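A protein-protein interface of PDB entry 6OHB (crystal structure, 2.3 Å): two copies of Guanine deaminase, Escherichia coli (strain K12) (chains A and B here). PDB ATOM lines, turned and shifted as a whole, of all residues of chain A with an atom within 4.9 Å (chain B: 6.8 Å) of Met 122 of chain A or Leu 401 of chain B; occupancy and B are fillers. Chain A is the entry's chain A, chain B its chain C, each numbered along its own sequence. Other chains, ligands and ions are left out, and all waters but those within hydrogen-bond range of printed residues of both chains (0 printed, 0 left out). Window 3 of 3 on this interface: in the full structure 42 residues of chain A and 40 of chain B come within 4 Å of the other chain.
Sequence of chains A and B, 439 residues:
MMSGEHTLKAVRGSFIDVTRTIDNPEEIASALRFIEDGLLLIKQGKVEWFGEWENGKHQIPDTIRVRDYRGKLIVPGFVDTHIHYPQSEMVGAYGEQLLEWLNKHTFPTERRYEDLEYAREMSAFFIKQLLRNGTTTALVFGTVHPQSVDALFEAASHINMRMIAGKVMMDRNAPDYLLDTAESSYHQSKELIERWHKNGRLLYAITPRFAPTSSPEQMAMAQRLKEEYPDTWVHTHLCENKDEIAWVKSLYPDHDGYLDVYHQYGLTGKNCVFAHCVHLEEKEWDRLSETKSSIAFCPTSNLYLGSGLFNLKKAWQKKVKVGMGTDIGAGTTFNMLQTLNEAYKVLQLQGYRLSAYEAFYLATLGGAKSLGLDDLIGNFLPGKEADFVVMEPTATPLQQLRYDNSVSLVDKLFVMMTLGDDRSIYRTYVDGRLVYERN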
ATOM      1  N   TYR A  85      22.130 -29.398  25.868  1.00  0.00           N
ATOM      2  CA  TYR A  85      21.354 -28.586  24.928  1.00  0.00           C
ATOM      3  C   TYR A  85      20.512 -27.488  25.584  1.00  0.00           C
ATOM      4  O   TYR A  85      20.574 -26.336  25.116  1.00  0.00           O
ATOM      5  CB  TYR A  85      20.505 -29.526  24.056  1.00  0.00           C
ATOM      6  CG  TYR A  85      19.113 -29.050  23.666  1.00  0.00           C
ATOM      7  CD1 TYR A  85      18.927 -27.919  22.871  1.00  0.00           C
ATOM      8  CD2 TYR A  85      17.983 -29.762  24.063  1.00  0.00           C
ATOM      9  CE1 TYR A  85      17.658 -27.498  22.510  1.00  0.00           C
ATOM     10  CE2 TYR A  85      16.707 -29.348  23.702  1.00  0.00           C
ATOM     11  CZ  TYR A  85      16.551 -28.218  22.927  1.00  0.00           C
ATOM     12  OH  TYR A  85      15.284 -27.807  22.570  1.00  0.00           O
ATOM     13  N   SER A  88      21.973 -23.046  27.117  1.00  0.00           N
ATOM     14  CA  SER A  88      22.828 -22.035  26.503  1.00  0.00           C
ATOM     15  C   SER A  88      22.663 -20.670  27.168  1.00  0.00           C
ATOM     16  O   SER A  88      23.638 -19.922  27.310  1.00  0.00           O
ATOM     17  CB  SER A  88      22.529 -21.938  25.006  1.00  0.00           C
ATOM     18  OG  SER A  88      22.775 -23.171  24.352  1.00  0.00           O
ATOM     19  N   GLU A  89      21.447 -20.334  27.596  1.00  0.00           N
ATOM     20  CA  GLU A  89      21.154 -19.011  28.136  1.00  0.00           C
ATOM     21  C   GLU A  89      21.469 -18.873  29.622  1.00  0.00           C
ATOM     22  O   GLU A  89      21.348 -17.768  30.161  1.00  0.00           O
ATOM     23  CB  GLU A  89      19.680 -18.659  27.891  1.00  0.00           C
ATOM     24  CG  GLU A  89      18.689 -19.511  28.669  1.00  0.00           C
ATOM     25  CD  GLU A  89      18.201 -20.720  27.886  1.00  0.00           C
ATOM     26  OE1 GLU A  89      19.028 -21.380  27.216  1.00  0.00           O
ATOM     27  OE2 GLU A  89      16.986 -21.010  27.940  1.00  0.00           O
ATOM     28  N   TYR A 113      12.008 -25.168  28.688  1.00  0.00           N
ATOM     29  CA  TYR A 113      11.991 -25.996  27.491  1.00  0.00           C
ATOM     30  C   TYR A 113      10.781 -26.926  27.419  1.00  0.00           C
ATOM     31  O   TYR A 113      10.756 -27.823  26.566  1.00  0.00           O
ATOM     32  CB  TYR A 113      13.300 -26.785  27.393  1.00  0.00           C
ATOM     33  CG  TYR A 113      14.470 -25.888  27.039  1.00  0.00           C
ATOM     34  CD1 TYR A 113      15.095 -25.114  28.007  1.00  0.00           C
ATOM     35  CD2 TYR A 113      14.921 -25.786  25.732  1.00  0.00           C
ATOM     36  CE1 TYR A 113      16.146 -24.279  27.686  1.00  0.00           C
ATOM     37  CE2 TYR A 113      15.973 -24.956  25.401  1.00  0.00           C
ATOM     38  CZ  TYR A 113      16.581 -24.202  26.380  1.00  0.00           C
ATOM     39  OH  TYR A 113      17.631 -23.373  26.054  1.00  0.00           O
ATOM     40  N   TYR A 118       9.671 -22.608  21.915  1.00  0.00           N
ATOM     41  CA  TYR A 118      10.953 -22.224  22.493  1.00  0.00           C
ATOM     42  C   TYR A 118      11.990 -23.325  22.308  1.00  0.00           C
ATOM     43  O   TYR A 118      13.161 -23.042  22.026  1.00  0.00           O
ATOM     44  CB  TYR A 118      10.785 -21.875  23.974  1.00  0.00           C
ATOM     45  CG  TYR A 118      12.034 -21.292  24.620  1.00  0.00           C
ATOM     46  CD1 TYR A 118      12.464 -20.006  24.314  1.00  0.00           C
ATOM     47  CD2 TYR A 118      12.779 -22.026  25.536  1.00  0.00           C
ATOM     48  CE1 TYR A 118      13.604 -19.470  24.901  1.00  0.00           C
ATOM     49  CE2 TYR A 118      13.920 -21.498  26.128  1.00  0.00           C
ATOM     50  CZ  TYR A 118      14.326 -20.221  25.806  1.00  0.00           C
ATOM     51  OH  TYR A 118      15.456 -19.694  26.388  1.00  0.00           O
ATOM     52  N   ALA A 119      11.583 -24.587  22.470  1.00  0.00           N
ATOM     53  CA  ALA A 119      12.519 -25.686  22.265  1.00  0.00           C
ATOM     54  C   ALA A 119      13.015 -25.729  20.825  1.00  0.00           C
ATOM     55  O   ALA A 119      14.201 -25.968  20.584  1.00  0.00           O
ATOM     56  CB  ALA A 119      11.876 -27.016  22.657  1.00  0.00           C
ATOM     57  N   ARG A 120      12.124 -25.493  19.856  1.00  0.00           N
ATOM     58  CA  ARG A 120      12.540 -25.462  18.455  1.00  0.00           C
ATOM     59  C   ARG A 120      13.533 -24.332  18.204  1.00  0.00           C
ATOM     60  O   ARG A 120      14.583 -24.530  17.569  1.00  0.00           O
ATOM     61  CB  ARG A 120      11.315 -25.322  17.550  1.00  0.00           C
ATOM     62  N   GLU A 121      13.202 -23.130  18.686  1.00  0.00           N
ATOM     63  CA  GLU A 121      14.090 -21.982  18.519  1.00  0.00           C
ATOM     64  C   GLU A 121      15.474 -22.268  19.096  1.00  0.00           C
ATOM     65  O   GLU A 121      16.502 -22.044  18.436  1.00  0.00           O
ATOM     66  CB  GLU A 121      13.466 -20.751  19.182  1.00  0.00           C
ATOM     67  CG  GLU A 121      14.155 -19.438  18.852  1.00  0.00           C
ATOM     68  CD  GLU A 121      13.644 -18.279  19.696  1.00  0.00           C
ATOM     69  OE1 GLU A 121      12.604 -18.446  20.368  1.00  0.00           O
ATOM     70  OE2 GLU A 121      14.286 -17.206  19.697  1.00  0.00           O
ATOM     71  N   MET A 122      15.523 -22.793  20.321  1.00  0.00           N
ATOM     72  CA  MET A 122      16.809 -23.040  20.952  1.00  0.00           C
ATOM     73  C   MET A 122      17.523 -24.239  20.346  1.00  0.00           C
ATOM     74  O   MET A 122      18.753 -24.302  20.398  1.00  0.00           O
ATOM     75  CB  MET A 122      16.632 -23.230  22.456  1.00  0.00           C
ATOM     76  CG  MET A 122      16.105 -21.986  23.174  1.00  0.00           C
ATOM     77  SD  MET A 122      16.980 -20.471  22.727  1.00  0.00           S
ATOM     78  CE  MET A 122      18.531 -20.701  23.600  1.00  0.00           C
ATOM     79  N   SER A 123      16.789 -25.168  19.734  1.00  0.00           N
ATOM     80  CA  SER A 123      17.433 -26.269  19.029  1.00  0.00           C
ATOM     81  C   SER A 123      18.178 -25.758  17.805  1.00  0.00           C
ATOM     82  O   SER A 123      19.330 -26.149  17.553  1.00  0.00           O
ATOM     83  CB  SER A 123      16.386 -27.309  18.630  1.00  0.00           C
ATOM     84  N   ALA A 124      17.535 -24.866  17.044  1.00  0.00           N
ATOM     85  CA  ALA A 124      18.220 -24.222  15.926  1.00  0.00           C
ATOM     86  C   ALA A 124      19.439 -23.438  16.405  1.00  0.00           C
ATOM     87  O   ALA A 124      20.529 -23.544  15.822  1.00  0.00           O
ATOM     88  CB  ALA A 124      17.254 -23.312  15.164  1.00  0.00           C
ATOM     89  N   PHE A 125      19.277 -22.654  17.478  1.00  0.00           N
ATOM     90  CA  PHE A 125      20.401 -21.880  18.011  1.00  0.00           C
ATOM     91  C   PHE A 125      21.556 -22.785  18.433  1.00  0.00           C
ATOM     92  O   PHE A 125      22.729 -22.476  18.179  1.00  0.00           O
ATOM     93  CB  PHE A 125      19.930 -21.025  19.195  1.00  0.00           C
ATOM     94  CG  PHE A 125      21.032 -20.251  19.868  1.00  0.00           C
ATOM     95  CD1 PHE A 125      21.348 -18.972  19.453  1.00  0.00           C
ATOM     96  CD2 PHE A 125      21.750 -20.800  20.919  1.00  0.00           C
ATOM     97  CE1 PHE A 125      22.365 -18.255  20.069  1.00  0.00           C
ATOM     98  CE2 PHE A 125      22.766 -20.088  21.536  1.00  0.00           C
ATOM     99  CZ  PHE A 125      23.073 -18.814  21.109  1.00  0.00           C
ATOM    100  N   PHE A 126      21.238 -23.905  19.084  1.00  0.00           N
ATOM    101  CA  PHE A 126      22.257 -24.830  19.567  1.00  0.00           C
ATOM    102  C   PHE A 126      23.031 -25.447  18.406  1.00  0.00           C
ATOM    103  O   PHE A 126      24.268 -25.535  18.448  1.00  0.00           O
ATOM    104  CB  PHE A 126      21.575 -25.903  20.420  1.00  0.00           C
ATOM    105  CG  PHE A 126      22.508 -26.909  21.016  1.00  0.00           C
ATOM    106  CD1 PHE A 126      23.146 -26.654  22.221  1.00  0.00           C
ATOM    107  CD2 PHE A 126      22.715 -28.127  20.394  1.00  0.00           C
ATOM    108  CE1 PHE A 126      23.997 -27.593  22.784  1.00  0.00           C
ATOM    109  CE2 PHE A 126      23.563 -29.072  20.946  1.00  0.00           C
ATOM    110  CZ  PHE A 126      24.206 -28.810  22.140  1.00  0.00           C
ATOM    111  N   PRO B 393      27.926  -5.321  25.057  1.00  0.00           N
ATOM    112  CA  PRO B 393      27.715  -6.610  25.728  1.00  0.00           C
ATOM    113  C   PRO B 393      27.021  -7.639  24.868  1.00  0.00           C
ATOM    114  O   PRO B 393      26.990  -8.815  25.250  1.00  0.00           O
ATOM    115  CB  PRO B 393      26.847  -6.232  26.929  1.00  0.00           C
ATOM    116  CG  PRO B 393      26.125  -5.000  26.505  1.00  0.00           C
ATOM    117  CD  PRO B 393      27.049  -4.259  25.584  1.00  0.00           C
ATOM    118  N   THR B 394      26.475  -7.240  23.723  1.00  0.00           N
ATOM    119  CA  THR B 394      25.774  -8.137  22.816  1.00  0.00           C
ATOM    120  C   THR B 394      26.601  -8.446  21.569  1.00  0.00           C
ATOM    121  O   THR B 394      26.047  -8.655  20.486  1.00  0.00           O
ATOM    122  CB  THR B 394      24.417  -7.540  22.443  1.00  0.00           C
ATOM    123  OG1 THR B 394      24.587  -6.181  22.023  1.00  0.00           O
ATOM    124  CG2 THR B 394      23.476  -7.580  23.641  1.00  0.00           C
ATOM    125  N   THR B 396      28.540 -10.980  20.699  1.00  0.00           N
ATOM    126  CA  THR B 396      28.586 -12.366  20.250  1.00  0.00           C
ATOM    127  C   THR B 396      27.249 -13.047  20.519  1.00  0.00           C
ATOM    128  O   THR B 396      26.566 -12.702  21.486  1.00  0.00           O
ATOM    129  CB  THR B 396      29.745 -13.099  20.963  1.00  0.00           C
ATOM    130  OG1 THR B 396      30.984 -12.812  20.295  1.00  0.00           O
ATOM    131  CG2 THR B 396      29.534 -14.609  21.086  1.00  0.00           C
ATOM    132  N   PRO B 397      26.841 -14.008  19.668  1.00  0.00           N
ATOM    133  CA  PRO B 397      25.516 -14.638  19.856  1.00  0.00           C
ATOM    134  C   PRO B 397      25.265 -15.222  21.240  1.00  0.00           C
ATOM    135  O   PRO B 397      24.201 -14.979  21.826  1.00  0.00           O
ATOM    136  CB  PRO B 397      25.502 -15.729  18.765  1.00  0.00           C
ATOM    137  CG  PRO B 397      26.953 -15.895  18.351  1.00  0.00           C
ATOM    138  CD  PRO B 397      27.496 -14.505  18.446  1.00  0.00           C
ATOM    139  N   LEU B 398      26.215 -15.988  21.786  1.00  0.00           N
ATOM    140  CA  LEU B 398      26.033 -16.515  23.134  1.00  0.00           C
ATOM    141  C   LEU B 398      26.075 -15.400  24.171  1.00  0.00           C
ATOM    142  O   LEU B 398      25.279 -15.393  25.123  1.00  0.00           O
ATOM    143  CB  LEU B 398      27.095 -17.568  23.444  1.00  0.00           C
ATOM    144  CG  LEU B 398      26.861 -18.313  24.762  1.00  0.00           C
ATOM    145  CD1 LEU B 398      25.595 -19.157  24.687  1.00  0.00           C
ATOM    146  CD2 LEU B 398      28.057 -19.173  25.151  1.00  0.00           C
ATOM    147  N   GLN B 399      27.005 -14.456  24.008  1.00  0.00           N
ATOM    148  CA  GLN B 399      27.078 -13.333  24.933  1.00  0.00           C
ATOM    149  C   GLN B 399      25.792 -12.524  24.896  1.00  0.00           C
ATOM    150  O   GLN B 399      25.263 -12.139  25.942  1.00  0.00           O
ATOM    151  CB  GLN B 399      28.284 -12.453  24.606  1.00  0.00           C
ATOM    152  CG  GLN B 399      28.636 -11.476  25.720  1.00  0.00           C
ATOM    153  CD  GLN B 399      29.950 -10.754  25.484  1.00  0.00           C
ATOM    154  OE1 GLN B 399      30.440 -10.681  24.355  1.00  0.00           O
ATOM    155  NE2 GLN B 399      30.529 -10.220  26.554  1.00  0.00           N
ATOM    156  N   GLN B 400      25.273 -12.261  23.697  1.00  0.00           N
ATOM    157  CA  GLN B 400      24.019 -11.529  23.582  1.00  0.00           C
ATOM    158  C   GLN B 400      22.872 -12.303  24.219  1.00  0.00           C
ATOM    159  O   GLN B 400      22.041 -11.722  24.926  1.00  0.00           O
ATOM    160  CB  GLN B 400      23.721 -11.221  22.113  1.00  0.00           C
ATOM    161  CG  GLN B 400      22.321 -10.670  21.858  1.00  0.00           C
ATOM    162  CD  GLN B 400      22.223  -9.862  20.570  1.00  0.00           C
ATOM    163  OE1 GLN B 400      22.900 -10.153  19.579  1.00  0.00           O
ATOM    164  NE2 GLN B 400      21.372  -8.840  20.579  1.00  0.00           N
ATOM    165  N   LEU B 401      22.814 -13.616  23.988  1.00  0.00           N
ATOM    166  CA  LEU B 401      21.731 -14.417  24.552  1.00  0.00           C
ATOM    167  C   LEU B 401      21.749 -14.374  26.075  1.00  0.00           C
ATOM    168  O   LEU B 401      20.696 -14.261  26.712  1.00  0.00           O
ATOM    169  CB  LEU B 401      21.828 -15.860  24.057  1.00  0.00           C
ATOM    170  CG  LEU B 401      20.766 -16.831  24.587  1.00  0.00           C
ATOM    171  CD1 LEU B 401      19.414 -16.548  23.950  1.00  0.00           C
ATOM    172  CD2 LEU B 401      21.180 -18.281  24.349  1.00  0.00           C
ATOM    173  N   ARG B 402      22.937 -14.459  26.677  1.00  0.00           N
ATOM    174  CA  ARG B 402      23.026 -14.438  28.134  1.00  0.00           C
ATOM    175  C   ARG B 402      22.823 -13.037  28.698  1.00  0.00           C
ATOM    176  O   ARG B 402      22.323 -12.886  29.819  1.00  0.00           O
ATOM    177  CB  ARG B 402      24.371 -15.004  28.579  1.00  0.00           C
ATOM    178  CG  ARG B 402      24.568 -16.456  28.174  1.00  0.00           C
ATOM    179  CD  ARG B 402      25.708 -17.093  28.934  1.00  0.00           C
ATOM    180  NE  ARG B 402      25.578 -18.543  28.961  1.00  0.00           N
ATOM    181  CZ  ARG B 402      26.365 -19.350  29.662  1.00  0.00           C
ATOM    182  NH1 ARG B 402      27.343 -18.844  30.397  1.00  0.00           N
ATOM    183  NH2 ARG B 402      26.170 -20.660  29.627  1.00  0.00           N
ATOM    184  N   TYR B 403      23.200 -12.008  27.939  1.00  0.00           N
ATOM    185  CA  TYR B 403      22.962 -10.639  28.367  1.00  0.00           C
ATOM    186  C   TYR B 403      21.488 -10.274  28.244  1.00  0.00           C
ATOM    187  O   TYR B 403      20.943  -9.574  29.108  1.00  0.00           O
ATOM    188  CB  TYR B 403      23.826  -9.686  27.546  1.00  0.00           C
ATOM    189  CG  TYR B 403      23.877  -8.282  28.089  1.00  0.00           C
ATOM    190  CD1 TYR B 403      24.832  -7.920  29.025  1.00  0.00           C
ATOM    191  CD2 TYR B 403      22.970  -7.316  27.665  1.00  0.00           C
ATOM    192  CE1 TYR B 403      24.885  -6.629  29.528  1.00  0.00           C
ATOM    193  CE2 TYR B 403      23.016  -6.024  28.159  1.00  0.00           C
ATOM    194  CZ  TYR B 403      23.977  -5.686  29.090  1.00  0.00           C
ATOM    195  OH  TYR B 403      24.032  -4.402  29.588  1.00  0.00           O
ATOM    196  N   ASP B 404      20.823 -10.742  27.183  1.00  0.00           N
ATOM    197  CA  ASP B 404      19.387 -10.524  27.048  1.00  0.00           C
ATOM    198  C   ASP B 404      18.605 -11.149  28.194  1.00  0.00           C
ATOM    199  O   ASP B 404      17.458 -10.761  28.430  1.00  0.00           O
ATOM    200  CB  ASP B 404      18.866 -11.101  25.726  1.00  0.00           C
ATOM    201  CG  ASP B 404      19.431 -10.397  24.503  1.00  0.00           C
ATOM    202  OD1 ASP B 404      20.027  -9.307  24.650  1.00  0.00           O
ATOM    203  OD2 ASP B 404      19.280 -10.945  23.387  1.00  0.00           O
ATOM    204  N   ASN B 405      19.188 -12.118  28.894  1.00  0.00           N
ATOM    205  CA  ASN B 405      18.535 -12.776  30.015  1.00  0.00           C
ATOM    206  C   ASN B 405      19.045 -12.298  31.367  1.00  0.00           C
ATOM    207  O   ASN B 405      18.659 -12.868  32.392  1.00  0.00           O
ATOM    208  CB  ASN B 405      18.708 -14.293  29.907  1.00  0.00           C
ATOM    209  CG  ASN B 405      17.640 -14.933  29.052  1.00  0.00           C
ATOM    210  OD1 ASN B 405      16.473 -14.996  29.443  1.00  0.00           O
ATOM    211  ND2 ASN B 405      18.028 -15.401  27.869  1.00  0.00           N
ATOM    212  N   SER B 406      19.931 -11.307  31.392  1.00  0.00           N
ATOM    213  CA  SER B 406      20.406 -10.709  32.631  1.00  0.00           C
ATOM    214  C   SER B 406      19.666  -9.404  32.888  1.00  0.00           C
ATOM    215  O   SER B 406      19.650  -8.519  32.026  1.00  0.00           O
ATOM    216  CB  SER B 406      21.914 -10.455  32.561  1.00  0.00           C
ATOM    217  OG  SER B 406      22.616 -11.632  32.213  1.00  0.00           O
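OE1 of Glu 89 of chain A lies within hydrogen-bond range of OH of Tyr 113 of chain A (2.7 Å). The side-chain carboxylate (OE2) of Glu 89 of chain A sits at hydrogen-bond distance from the side-chain hydroxyl (OH) of Tyr 118 of chain A (2.5 Å). The backbone carbonyl oxygen of Leu 401 of chain B is in hydrogen-bond range of the side-chain amide nitrogen of Asn 405 of chain B (3.1 Å). O of Arg 402 of chain B sits at hydrogen-bond distance from OG of Ser 406 of chain B.
No position is printed for both chains.
Of chain B, only Leu 401 (3.7 Å) comes within 4 Å of Met 122 of chain A. Of the printed residues of chain B, Phe 125 of chain A touches Leu 401. Of the printed residues of chain A, Leu 398 of chain B touches Ser 88 (3.4 Å). Of the printed residues of chain A, Arg 402 of chain B touches Ser 88 (2.9 Å). Tyr 403 of chain B touches none of the printed residues of chain A. Of the printed residues of chain A, Asn 405 of chain B touches Glu 89. Ser 406 of chain B touches none of the printed residues of chain A. The nearest printed residue of chain B that does not touch Met 122 of chain A is Asn 405 of chain B (6.8 Å).
NE of Arg 402 of chain B is in hydrogen-bond range of O of Ser 88 of chain A.
Among the printed residues, pairs that only touch across the chains: Ser 88 of chain A with Leu 398 of chain B, Glu 89 of chain A with Asn 405 of chain B, Met 122 of chain A with Leu 401 of chain B, Phe 125 of chain A with Leu 401 of chain B, Glu 89 of chain A with Leu 401 of chain B and Ser 88 of chain A with Leu 401 of chain B.
Printed residues of chain A that touch a printed residue of chain B: Ser 88, Glu 89, Met 122 and Phe 125. Hydrophobic or aromatic side chains of chain A within 4 Å of the printed part of chain B: Met 122 and Phe 125. Printed residues of chain B that touch a printed residue of chain A: Leu 398, Leu 401, Arg 402 and Asn 405.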
